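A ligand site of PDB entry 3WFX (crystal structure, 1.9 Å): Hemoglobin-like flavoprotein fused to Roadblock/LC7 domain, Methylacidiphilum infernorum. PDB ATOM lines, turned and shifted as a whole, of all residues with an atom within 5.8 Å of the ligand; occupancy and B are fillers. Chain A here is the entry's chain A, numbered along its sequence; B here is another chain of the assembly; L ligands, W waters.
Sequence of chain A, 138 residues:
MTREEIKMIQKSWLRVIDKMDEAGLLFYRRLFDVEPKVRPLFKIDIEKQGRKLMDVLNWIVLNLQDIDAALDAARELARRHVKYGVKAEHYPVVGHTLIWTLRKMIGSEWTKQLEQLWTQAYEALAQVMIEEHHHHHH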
ATOM      1  N   LEU A  77      20.335   8.520 -28.939  1.00  0.00           N
ATOM      2  CA  LEU A  77      20.059   7.158 -28.470  1.00  0.00           C
ATOM      3  C   LEU A  77      19.544   6.293 -29.609  1.00  0.00           C
ATOM      4  O   LEU A  77      19.951   5.123 -29.758  1.00  0.00           O
ATOM      5  CB  LEU A  77      19.049   7.190 -27.320  1.00  0.00           C
ATOM      6  CG  LEU A  77      18.651   5.812 -26.741  1.00  0.00           C
ATOM      7  CD1 LEU A  77      19.839   5.181 -26.015  1.00  0.00           C
ATOM      8  CD2 LEU A  77      17.481   5.956 -25.800  1.00  0.00           C
ATOM      9  N   ARG A  80      22.291   5.103 -31.989  1.00  0.00           N
ATOM     10  CA  ARG A  80      22.981   3.913 -31.456  1.00  0.00           C
ATOM     11  C   ARG A  80      22.149   2.649 -31.684  1.00  0.00           C
ATOM     12  O   ARG A  80      22.670   1.596 -32.045  1.00  0.00           O
ATOM     13  CB  ARG A  80      23.336   4.079 -29.980  1.00  0.00           C
ATOM     14  CG  ARG A  80      24.282   5.281 -29.692  1.00  0.00           C
ATOM     15  CD  ARG A  80      24.945   5.139 -28.318  1.00  0.00           C
ATOM     16  NE  ARG A  80      24.032   5.294 -27.178  1.00  0.00           N
ATOM     17  CZ  ARG A  80      23.727   6.481 -26.638  1.00  0.00           C
ATOM     18  NH1 ARG A  80      24.246   7.583 -27.143  1.00  0.00           N
ATOM     19  NH2 ARG A  80      22.907   6.566 -25.603  1.00  0.00           N
ATOM     20  N   HIS A  81      20.836   2.750 -31.484  1.00  0.00           N
ATOM     21  CA  HIS A  81      19.946   1.620 -31.709  1.00  0.00           C
ATOM     22  C   HIS A  81      19.873   1.184 -33.157  1.00  0.00           C
ATOM     23  O   HIS A  81      19.782  -0.015 -33.428  1.00  0.00           O
ATOM     24  CB  HIS A  81      18.554   1.921 -31.166  1.00  0.00           C
ATOM     25  CG  HIS A  81      18.449   1.764 -29.689  1.00  0.00           C
ATOM     26  ND1 HIS A  81      19.080   2.613 -28.804  1.00  0.00           N
ATOM     27  CD2 HIS A  81      17.854   0.814 -28.934  1.00  0.00           C
ATOM     28  CE1 HIS A  81      18.857   2.209 -27.571  1.00  0.00           C
ATOM     29  NE2 HIS A  81      18.116   1.118 -27.628  1.00  0.00           N
ATOM     30  N   TYR A  84      22.637  -0.962 -33.479  1.00  0.00           N
ATOM     31  CA  TYR A  84      22.417  -2.274 -32.833  1.00  0.00           C
ATOM     32  C   TYR A  84      21.519  -3.195 -33.682  1.00  0.00           C
ATOM     33  O   TYR A  84      21.394  -4.371 -33.394  1.00  0.00           O
ATOM     34  CB  TYR A  84      21.756  -2.122 -31.462  1.00  0.00           C
ATOM     35  CG  TYR A  84      22.473  -1.221 -30.475  1.00  0.00           C
ATOM     36  CD1 TYR A  84      23.844  -1.037 -30.530  1.00  0.00           C
ATOM     37  CD2 TYR A  84      21.765  -0.563 -29.486  1.00  0.00           C
ATOM     38  CE1 TYR A  84      24.493  -0.219 -29.623  1.00  0.00           C
ATOM     39  CE2 TYR A  84      22.390   0.249 -28.568  1.00  0.00           C
ATOM     40  CZ  TYR A  84      23.760   0.427 -28.645  1.00  0.00           C
ATOM     41  OH  TYR A  84      24.369   1.252 -27.736  1.00  0.00           O
ATOM     42  N   VAL A  86      18.242  -2.471 -34.233  1.00  0.00           N
ATOM     43  CA  VAL A  86      16.850  -2.241 -33.861  1.00  0.00           C
ATOM     44  C   VAL A  86      16.134  -1.568 -35.012  1.00  0.00           C
ATOM     45  O   VAL A  86      16.732  -0.764 -35.739  1.00  0.00           O
ATOM     46  CB  VAL A  86      16.744  -1.378 -32.584  1.00  0.00           C
ATOM     47  CG1 VAL A  86      15.289  -1.062 -32.250  1.00  0.00           C
ATOM     48  CG2 VAL A  86      17.437  -2.089 -31.418  1.00  0.00           C
ATOM     49  N   LYS A  87      14.864  -1.899 -35.183  1.00  0.00           N
ATOM     50  CA  LYS A  87      14.044  -1.259 -36.191  1.00  0.00           C
ATOM     51  C   LYS A  87      12.790  -0.599 -35.585  1.00  0.00           C
ATOM     52  O   LYS A  87      12.416  -0.888 -34.445  1.00  0.00           O
ATOM     53  CB  LYS A  87      13.693  -2.253 -37.306  1.00  0.00           C
ATOM     54  CG  LYS A  87      14.900  -2.519 -38.218  1.00  0.00           C
ATOM     55  CD  LYS A  87      14.625  -3.576 -39.269  1.00  0.00           C
ATOM     56  CE  LYS A  87      15.596  -3.435 -40.421  1.00  0.00           C
ATOM     57  NZ  LYS A  87      17.000  -3.213 -39.953  1.00  0.00           N
ATOM     58  N   HIS A  90      10.053  -2.529 -33.786  1.00  0.00           N
ATOM     59  CA  HIS A  90      10.358  -3.256 -32.536  1.00  0.00           C
ATOM     60  C   HIS A  90       9.927  -2.507 -31.291  1.00  0.00           C
ATOM     61  O   HIS A  90       9.820  -3.086 -30.207  1.00  0.00           O
ATOM     62  CB  HIS A  90      11.857  -3.526 -32.408  1.00  0.00           C
ATOM     63  CG  HIS A  90      12.411  -4.457 -33.444  1.00  0.00           C
ATOM     64  ND1 HIS A  90      13.678  -4.290 -33.969  1.00  0.00           N
ATOM     65  CD2 HIS A  90      11.911  -5.583 -33.995  1.00  0.00           C
ATOM     66  CE1 HIS A  90      13.915  -5.262 -34.829  1.00  0.00           C
ATOM     67  NE2 HIS A  90      12.859  -6.059 -34.864  1.00  0.00           N
ATOM     68  N   TYR A  91       9.674  -1.212 -31.426  1.00  0.00           N
ATOM     69  CA  TYR A  91       9.377  -0.378 -30.259  1.00  0.00           C
ATOM     70  C   TYR A  91       8.105  -0.720 -29.486  1.00  0.00           C
ATOM     71  O   TYR A  91       8.103  -0.617 -28.252  1.00  0.00           O
ATOM     72  CB  TYR A  91       9.415   1.114 -30.609  1.00  0.00           C
ATOM     73  CG  TYR A  91      10.827   1.621 -30.754  1.00  0.00           C
ATOM     74  CD1 TYR A  91      11.477   2.239 -29.693  1.00  0.00           C
ATOM     75  CD2 TYR A  91      11.512   1.454 -31.935  1.00  0.00           C
ATOM     76  CE1 TYR A  91      12.768   2.700 -29.836  1.00  0.00           C
ATOM     77  CE2 TYR A  91      12.790   1.905 -32.094  1.00  0.00           C
ATOM     78  CZ  TYR A  91      13.412   2.534 -31.036  1.00  0.00           C
ATOM     79  OH  TYR A  91      14.709   2.956 -31.206  1.00  0.00           O
ATOM     80  N   VAL A  94       8.654  -3.723 -26.965  1.00  0.00           N
ATOM     81  CA  VAL A  94       9.509  -3.356 -25.860  1.00  0.00           C
ATOM     82  C   VAL A  94       8.729  -2.530 -24.845  1.00  0.00           C
ATOM     83  O   VAL A  94       8.805  -2.785 -23.650  1.00  0.00           O
ATOM     84  CB  VAL A  94      10.757  -2.589 -26.353  1.00  0.00           C
ATOM     85  CG1 VAL A  94      11.435  -1.876 -25.189  1.00  0.00           C
ATOM     86  CG2 VAL A  94      11.695  -3.581 -27.033  1.00  0.00           C
ATOM     87  N   LEU A  98       8.072  -3.540 -21.112  1.00  0.00           N
ATOM     88  CA  LEU A  98       8.463  -2.649 -20.024  1.00  0.00           C
ATOM     89  C   LEU A  98       7.283  -2.464 -19.080  1.00  0.00           C
ATOM     90  O   LEU A  98       7.426  -2.637 -17.884  1.00  0.00           O
ATOM     91  CB  LEU A  98       8.957  -1.301 -20.565  1.00  0.00           C
ATOM     92  CG  LEU A  98      10.352  -1.350 -21.164  1.00  0.00           C
ATOM     93  CD1 LEU A  98      10.713  -0.052 -21.897  1.00  0.00           C
ATOM     94  CD2 LEU A  98      11.379  -1.633 -20.081  1.00  0.00           C
ATOM     95  N   TYR A 122       6.713   6.602 -22.646  1.00  0.00           N
ATOM     96  CA  TYR A 122       7.324   5.691 -23.612  1.00  0.00           C
ATOM     97  C   TYR A 122       6.951   6.019 -25.044  1.00  0.00           C
ATOM     98  O   TYR A 122       7.819   6.055 -25.913  1.00  0.00           O
ATOM     99  CB  TYR A 122       6.957   4.239 -23.300  1.00  0.00           C
ATOM    100  CG  TYR A 122       7.694   3.270 -24.212  1.00  0.00           C
ATOM    101  CD1 TYR A 122       8.940   2.766 -23.859  1.00  0.00           C
ATOM    102  CD2 TYR A 122       7.154   2.912 -25.445  1.00  0.00           C
ATOM    103  CE1 TYR A 122       9.632   1.899 -24.702  1.00  0.00           C
ATOM    104  CE2 TYR A 122       7.842   2.039 -26.300  1.00  0.00           C
ATOM    105  CZ  TYR A 122       9.071   1.539 -25.912  1.00  0.00           C
ATOM    106  OH  TYR A 122       9.758   0.672 -26.746  1.00  0.00           O
ATOM    107  N   LEU A 125       8.626   9.278 -26.332  1.00  0.00           N
ATOM    108  CA  LEU A 125      10.038   9.018 -26.603  1.00  0.00           C
ATOM    109  C   LEU A 125      10.188   8.146 -27.858  1.00  0.00           C
ATOM    110  O   LEU A 125      10.964   8.482 -28.756  1.00  0.00           O
ATOM    111  CB  LEU A 125      10.711   8.334 -25.393  1.00  0.00           C
ATOM    112  CG  LEU A 125      12.171   7.904 -25.547  1.00  0.00           C
ATOM    113  CD1 LEU A 125      13.011   8.987 -26.164  1.00  0.00           C
ATOM    114  CD2 LEU A 125      12.753   7.490 -24.196  1.00  0.00           C
ATOM    115  N   ALA A 126       9.451   7.046 -27.912  1.00  0.00           N
ATOM    116  CA  ALA A 126       9.551   6.130 -29.054  1.00  0.00           C
ATOM    117  C   ALA A 126       9.206   6.860 -30.356  1.00  0.00           C
ATOM    118  O   ALA A 126       9.851   6.657 -31.375  1.00  0.00           O
ATOM    119  CB  ALA A 126       8.667   4.876 -28.863  1.00  0.00           C
ATOM    120  N   MET A 129      12.332   8.738 -31.343  1.00  0.00           N
ATOM    121  CA  MET A 129      13.341   7.760 -31.757  1.00  0.00           C
ATOM    122  C   MET A 129      12.972   7.129 -33.094  1.00  0.00           C
ATOM    123  O   MET A 129      13.821   6.991 -33.966  1.00  0.00           O
ATOM    124  CB  MET A 129      13.541   6.686 -30.690  1.00  0.00           C
ATOM    125  CG  MET A 129      14.131   7.231 -29.373  1.00  0.00           C
ATOM    126  SD  MET A 129      14.236   5.956 -28.099  1.00  0.00           S
ATOM    127  CE  MET A 129      15.670   5.017 -28.682  1.00  0.00           C
ATOM    128  N   TYR B  28      13.695  -9.604 -19.638  1.00  0.00           N
ATOM    129  CA  TYR B  28      14.315 -10.233 -20.794  1.00  0.00           C
ATOM    130  C   TYR B  28      13.696 -11.585 -21.079  1.00  0.00           C
ATOM    131  O   TYR B  28      13.536 -11.974 -22.239  1.00  0.00           O
ATOM    132  CB  TYR B  28      15.829 -10.299 -20.634  1.00  0.00           C
ATOM    133  CG  TYR B  28      16.449  -8.952 -20.882  1.00  0.00           C
ATOM    134  CD1 TYR B  28      16.554  -8.440 -22.160  1.00  0.00           C
ATOM    135  CD2 TYR B  28      16.888  -8.159 -19.816  1.00  0.00           C
ATOM    136  CE1 TYR B  28      17.107  -7.183 -22.397  1.00  0.00           C
ATOM    137  CE2 TYR B  28      17.430  -6.905 -20.048  1.00  0.00           C
ATOM    138  CZ  TYR B  28      17.537  -6.417 -21.334  1.00  0.00           C
ATOM    139  OH  TYR B  28      18.086  -5.166 -21.551  1.00  0.00           O
ATOM    140  N   LEU B  31      10.350 -10.587 -22.923  1.00  0.00           N
ATOM    141  CA  LEU B  31      10.647 -10.109 -24.273  1.00  0.00           C
ATOM    142  C   LEU B  31      10.989 -11.264 -25.220  1.00  0.00           C
ATOM    143  O   LEU B  31      10.491 -11.329 -26.340  1.00  0.00           O
ATOM    144  CB  LEU B  31      11.817  -9.104 -24.248  1.00  0.00           C
ATOM    145  CG  LEU B  31      12.121  -8.405 -25.572  1.00  0.00           C
ATOM    146  CD1 LEU B  31      10.890  -7.627 -26.033  1.00  0.00           C
ATOM    147  CD2 LEU B  31      13.339  -7.469 -25.462  1.00  0.00           C
ATOM    148  N   VAL B  38      13.933 -11.051 -31.822  1.00  0.00           N
ATOM    149  CA  VAL B  38      14.868  -9.994 -31.447  1.00  0.00           C
ATOM    150  C   VAL B  38      15.995 -10.466 -30.543  1.00  0.00           C
ATOM    151  O   VAL B  38      16.935  -9.727 -30.279  1.00  0.00           O
ATOM    152  CB  VAL B  38      14.159  -8.791 -30.768  1.00  0.00           C
ATOM    153  CG1 VAL B  38      13.119  -8.174 -31.711  1.00  0.00           C
ATOM    154  CG2 VAL B  38      13.556  -9.207 -29.447  1.00  0.00           C
ATOM    155  N   LEU B  41      19.741  -9.785 -31.163  1.00  0.00           N
ATOM    156  CA  LEU B  41      20.192  -8.393 -31.095  1.00  0.00           C
ATOM    157  C   LEU B  41      20.968  -8.117 -29.808  1.00  0.00           C
ATOM    158  O   LEU B  41      21.820  -7.231 -29.767  1.00  0.00           O
ATOM    159  CB  LEU B  41      19.006  -7.440 -31.196  1.00  0.00           C
ATOM    160  CG  LEU B  41      18.755  -6.735 -32.518  1.00  0.00           C
ATOM    161  CD1 LEU B  41      18.745  -7.707 -33.672  1.00  0.00           C
ATOM    162  CD2 LEU B  41      17.456  -5.965 -32.443  1.00  0.00           C
ATOM    163  N   PHE B  42      20.651  -8.866 -28.763  1.00  0.00           N
ATOM    164  CA  PHE B  42      21.178  -8.555 -27.442  1.00  0.00           C
ATOM    165  C   PHE B  42      22.447  -9.314 -27.121  1.00  0.00           C
ATOM    166  O   PHE B  42      22.616 -10.461 -27.529  1.00  0.00           O
ATOM    167  CB  PHE B  42      20.108  -8.827 -26.380  1.00  0.00           C
ATOM    168  CG  PHE B  42      18.945  -7.897 -26.478  1.00  0.00           C
ATOM    169  CD1 PHE B  42      17.910  -8.155 -27.345  1.00  0.00           C
ATOM    170  CD2 PHE B  42      18.924  -6.731 -25.735  1.00  0.00           C
ATOM    171  CE1 PHE B  42      16.838  -7.281 -27.451  1.00  0.00           C
ATOM    172  CE2 PHE B  42      17.860  -5.853 -25.837  1.00  0.00           C
ATOM    173  CZ  PHE B  42      16.816  -6.123 -26.696  1.00  0.00           C
ATOM    174  N   LYS B  43      23.341  -8.662 -26.392  1.00  0.00           N
ATOM    175  CA  LYS B  43      24.559  -9.328 -25.948  1.00  0.00           C
ATOM    176  C   LYS B  43      24.245 -10.267 -24.795  1.00  0.00           C
ATOM    177  O   LYS B  43      23.529  -9.904 -23.858  1.00  0.00           O
ATOM    178  CB  LYS B  43      25.634  -8.315 -25.569  1.00  0.00           C
ATOM    179  CG  LYS B  43      26.188  -7.565 -26.779  1.00  0.00           C
ATOM    180  CD  LYS B  43      26.952  -8.505 -27.703  1.00  0.00           C
ATOM    181  CE  LYS B  43      26.569  -8.300 -29.161  1.00  0.00           C
ATOM    182  NZ  LYS B  43      25.291  -8.984 -29.513  1.00  0.00           N
ATOM    183  N   LYS B  52      21.252  -3.720 -17.162  1.00  0.00           N
ATOM    184  CA  LYS B  52      20.817  -3.383 -18.514  1.00  0.00           C
ATOM    185  C   LYS B  52      19.428  -2.784 -18.532  1.00  0.00           C
ATOM    186  O   LYS B  52      19.192  -1.834 -19.281  1.00  0.00           O
ATOM    187  CB  LYS B  52      20.845  -4.604 -19.460  1.00  0.00           C
ATOM    188  CG  LYS B  52      22.194  -5.304 -19.594  1.00  0.00           C
ATOM    189  CD  LYS B  52      23.284  -4.360 -20.068  1.00  0.00           C
ATOM    190  CE  LYS B  52      24.288  -5.097 -20.954  1.00  0.00           C
ATOM    191  NZ  LYS B  52      24.913  -6.268 -20.264  1.00  0.00           N
ATOM    192  N   ASP B  55      19.646   0.830 -16.990  1.00  0.00           N
ATOM    193  CA  ASP B  55      20.094   1.847 -17.932  1.00  0.00           C
ATOM    194  C   ASP B  55      18.908   2.401 -18.739  1.00  0.00           C
ATOM    195  O   ASP B  55      18.826   3.600 -19.018  1.00  0.00           O
ATOM    196  CB  ASP B  55      21.114   1.264 -18.925  1.00  0.00           C
ATOM    197  CG  ASP B  55      22.448   0.946 -18.270  1.00  0.00           C
ATOM    198  OD1 ASP B  55      22.723   1.464 -17.167  1.00  0.00           O
ATOM    199  OD2 ASP B  55      23.247   0.188 -18.873  1.00  0.00           O
ATOM    200  N   VAL B  56      17.991   1.511 -19.100  1.00  0.00           N
ATOM    201  CA  VAL B  56      16.847   1.877 -19.924  1.00  0.00           C
ATOM    202  C   VAL B  56      15.899   2.757 -19.115  1.00  0.00           C
ATOM    203  O   VAL B  56      15.521   3.864 -19.548  1.00  0.00           O
ATOM    204  CB  VAL B  56      16.080   0.612 -20.443  1.00  0.00           C
ATOM    205  CG1 VAL B  56      14.943   1.029 -21.370  1.00  0.00           C
ATOM    206  CG2 VAL B  56      17.007  -0.312 -21.180  1.00  0.00           C
ATOM    207  N   TRP B  59      17.369   6.125 -18.244  1.00  0.00           N
ATOM    208  CA  TRP B  59      17.417   6.988 -19.417  1.00  0.00           C
ATOM    209  C   TRP B  59      16.065   7.646 -19.591  1.00  0.00           C
ATOM    210  O   TRP B  59      15.964   8.877 -19.725  1.00  0.00           O
ATOM    211  CB  TRP B  59      17.818   6.213 -20.674  1.00  0.00           C
ATOM    212  CG  TRP B  59      18.421   7.092 -21.729  1.00  0.00           C
ATOM    213  CD1 TRP B  59      19.741   7.216 -22.047  1.00  0.00           C
ATOM    214  CD2 TRP B  59      17.714   7.982 -22.596  1.00  0.00           C
ATOM    215  NE1 TRP B  59      19.899   8.134 -23.061  1.00  0.00           N
ATOM    216  CE2 TRP B  59      18.673   8.623 -23.414  1.00  0.00           C
ATOM    217  CE3 TRP B  59      16.363   8.307 -22.770  1.00  0.00           C
ATOM    218  CZ2 TRP B  59      18.322   9.542 -24.393  1.00  0.00           C
ATOM    219  CZ3 TRP B  59      16.021   9.230 -23.745  1.00  0.00           C
ATOM    220  CH2 TRP B  59      16.993   9.841 -24.531  1.00  0.00           C
ATOM    221  N   ILE B  60      15.015   6.834 -19.566  1.00  0.00           N
ATOM    222  CA  ILE B  60      13.653   7.342 -19.707  1.00  0.00           C
ATOM    223  C   ILE B  60      13.292   8.430 -18.695  1.00  0.00           C
ATOM    224  O   ILE B  60      12.842   9.513 -19.071  1.00  0.00           O
ATOM    225  CB  ILE B  60      12.635   6.185 -19.656  1.00  0.00           C
ATOM    226  CG1 ILE B  60      12.728   5.358 -20.943  1.00  0.00           C
ATOM    227  CG2 ILE B  60      11.225   6.708 -19.477  1.00  0.00           C
ATOM    228  CD1 ILE B  60      11.949   4.022 -20.872  1.00  0.00           C
HETATM  229  C1  LIG L   1      20.735  -0.725 -25.380  1.00  0.00           C
HETATM  230  C2  LIG L   1      17.359   2.435 -23.959  1.00  0.00           C
HETATM  231  C3  LIG L   1      14.314   0.564 -27.226  1.00  0.00           C
HETATM  232  C4  LIG L   1      17.351  -3.077 -28.039  1.00  0.00           C
HETATM  233  C5  LIG L   1      20.120   0.317 -24.730  1.00  0.00           C
HETATM  234  C6  LIG L   1      20.728   1.222 -23.773  1.00  0.00           C
HETATM  235  C7  LIG L   1      19.791   2.100 -23.381  1.00  0.00           C
HETATM  236  C8  LIG L   1      18.559   1.780 -24.080  1.00  0.00           C
HETATM  237  C9  LIG L   1      19.947   3.273 -22.387  1.00  0.00           C
HETATM  238  C10 LIG L   1      22.207   1.198 -23.300  1.00  0.00           C
HETATM  239  C11 LIG L   1      23.146   1.392 -24.496  1.00  0.00           C
HETATM  240  C12 LIG L   1      22.959   2.784 -25.043  1.00  0.00           C
HETATM  241  O1  LIG L   1      22.718   3.717 -24.237  1.00  0.00           O
HETATM  242  O2  LIG L   1      23.031   2.973 -26.283  1.00  0.00           O
HETATM  243  C13 LIG L   1      16.242   2.215 -24.736  1.00  0.00           C
HETATM  244  C14 LIG L   1      15.009   2.987 -24.707  1.00  0.00           C
HETATM  245  C15 LIG L   1      14.163   2.450 -25.602  1.00  0.00           C
HETATM  246  C16 LIG L   1      14.848   1.351 -26.236  1.00  0.00           C
HETATM  247  C17 LIG L   1      14.771   4.171 -23.758  1.00  0.00           C
HETATM  248  C18 LIG L   1      12.727   2.905 -25.985  1.00  0.00           C
HETATM  249  C19 LIG L   1      12.298   4.163 -25.889  1.00  0.00           C
HETATM  250  C20 LIG L   1      14.849  -0.589 -27.726  1.00  0.00           C
HETATM  251  C21 LIG L   1      14.188  -1.476 -28.665  1.00  0.00           C
HETATM  252  C22 LIG L   1      14.997  -2.515 -28.902  1.00  0.00           C
HETATM  253  C23 LIG L   1      16.220  -2.305 -28.107  1.00  0.00           C
HETATM  254  C24 LIG L   1      12.791  -1.237 -29.275  1.00  0.00           C
HETATM  255  C25 LIG L   1      14.617  -3.661 -29.882  1.00  0.00           C
HETATM  256  C26 LIG L   1      15.128  -4.882 -29.765  1.00  0.00           C
HETATM  257  C27 LIG L   1      18.572  -2.727 -27.492  1.00  0.00           C
HETATM  258  C28 LIG L   1      19.826  -3.437 -27.727  1.00  0.00           C
HETATM  259  C29 LIG L   1      20.877  -2.707 -26.899  1.00  0.00           C
HETATM  260  C30 LIG L   1      20.170  -1.623 -26.251  1.00  0.00           C
HETATM  261  C31 LIG L   1      20.069  -4.664 -28.637  1.00  0.00           C
HETATM  262  C32 LIG L   1      22.376  -3.050 -26.797  1.00  0.00           C
HETATM  263  C33 LIG L   1      22.645  -3.571 -25.396  1.00  0.00           C
HETATM  264  C34 LIG L   1      22.479  -5.074 -25.384  1.00  0.00           C
HETATM  265  O3  LIG L   1      23.024  -5.762 -26.292  1.00  0.00           O
HETATM  266  O4  LIG L   1      21.827  -5.594 -24.443  1.00  0.00           O
HETATM  267  N1  LIG L   1      18.808   0.686 -24.878  1.00  0.00           N
HETATM  268  N2  LIG L   1      16.104   1.236 -25.695  1.00  0.00           N
HETATM  269  N3  LIG L   1      16.077  -1.129 -27.400  1.00  0.00           N
HETATM  270  N4  LIG L   1      18.823  -1.670 -26.609  1.00  0.00           N
HETATM  271 FE1  LIG L   1      17.462  -0.230 -26.118  1.00  0.00          FE
HETATM  272  O   HOH W   1      20.515  -1.424 -21.693  1.00  0.00           O
HETATM  273  O   HOH W   2      22.918  -1.215 -21.272  1.00  0.00           O
HETATM  274  O   HOH W   3      23.106   4.614 -21.627  1.00  0.00           O
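OH of Tyr 84 sits at hydrogen-bond distance from O2 of the ligand.
NE of Arg 80 is in salt-bridge range of O2 of the ligand (2.7 Å).
The backbone NH (N) of Lys 43 of chain B sits at hydrogen-bond distance from an oxygen (O3) of the ligand (2.9 Å).
NE2 of His 81 binds FE1 of the ligand (2.1 Å).
Residues that only touch the ligand: Leu 77, Val 86, His 90, Tyr 91, Val 94, Tyr 122, Leu 125, Met 129, Leu 41 of chain B, Phe 42 of chain B, Asp 55 of chain B, Val 56 of chain B, Trp 59 of chain B and Ile 60 of chain B.
Hydrophobic or aromatic side chains within 4 Å of the ligand: Leu 77, His 81, Tyr 84, Val 86, His 90, Tyr 91, Val 94, Tyr 122, Leu 125, Met 129, Leu 41 of chain B, Phe 42 of chain B, Val 56 of chain B, Trp 59 of chain B and Ile 60 of chain B.
18 residues have an atom within 4 Å of the ligand: Leu 77, Arg 80, His 81, Tyr 84, Val 86, His 90, Tyr 91, Val 94, Tyr 122, Leu 125, Met 129, Leu 41 of chain B, Phe 42 of chain B, Lys 43 of chain B, Asp 55 of chain B, Val 56 of chain B, Trp 59 of chain B and Ile 60 of chain B.
The nearest printed residue that does not touch the ligand is Val 38 of chain B (4.2 Å).
O of His 81 lies within hydrogen-bond range of N of Val 86 (3.0 Å).
OH of Tyr 122 is in hydrogen-bond range of O of Tyr 91, at 2.6 Å.
The backbone NH of Lys 87 lies within hydrogen-bond range of a ring nitrogen (ND1) of His 90, at 2.9 Å.
The backbone carbonyl oxygen (O) of Leu 77 is in hydrogen-bond range of a ring nitrogen (ND1) of His 81, 2.8 Å away.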
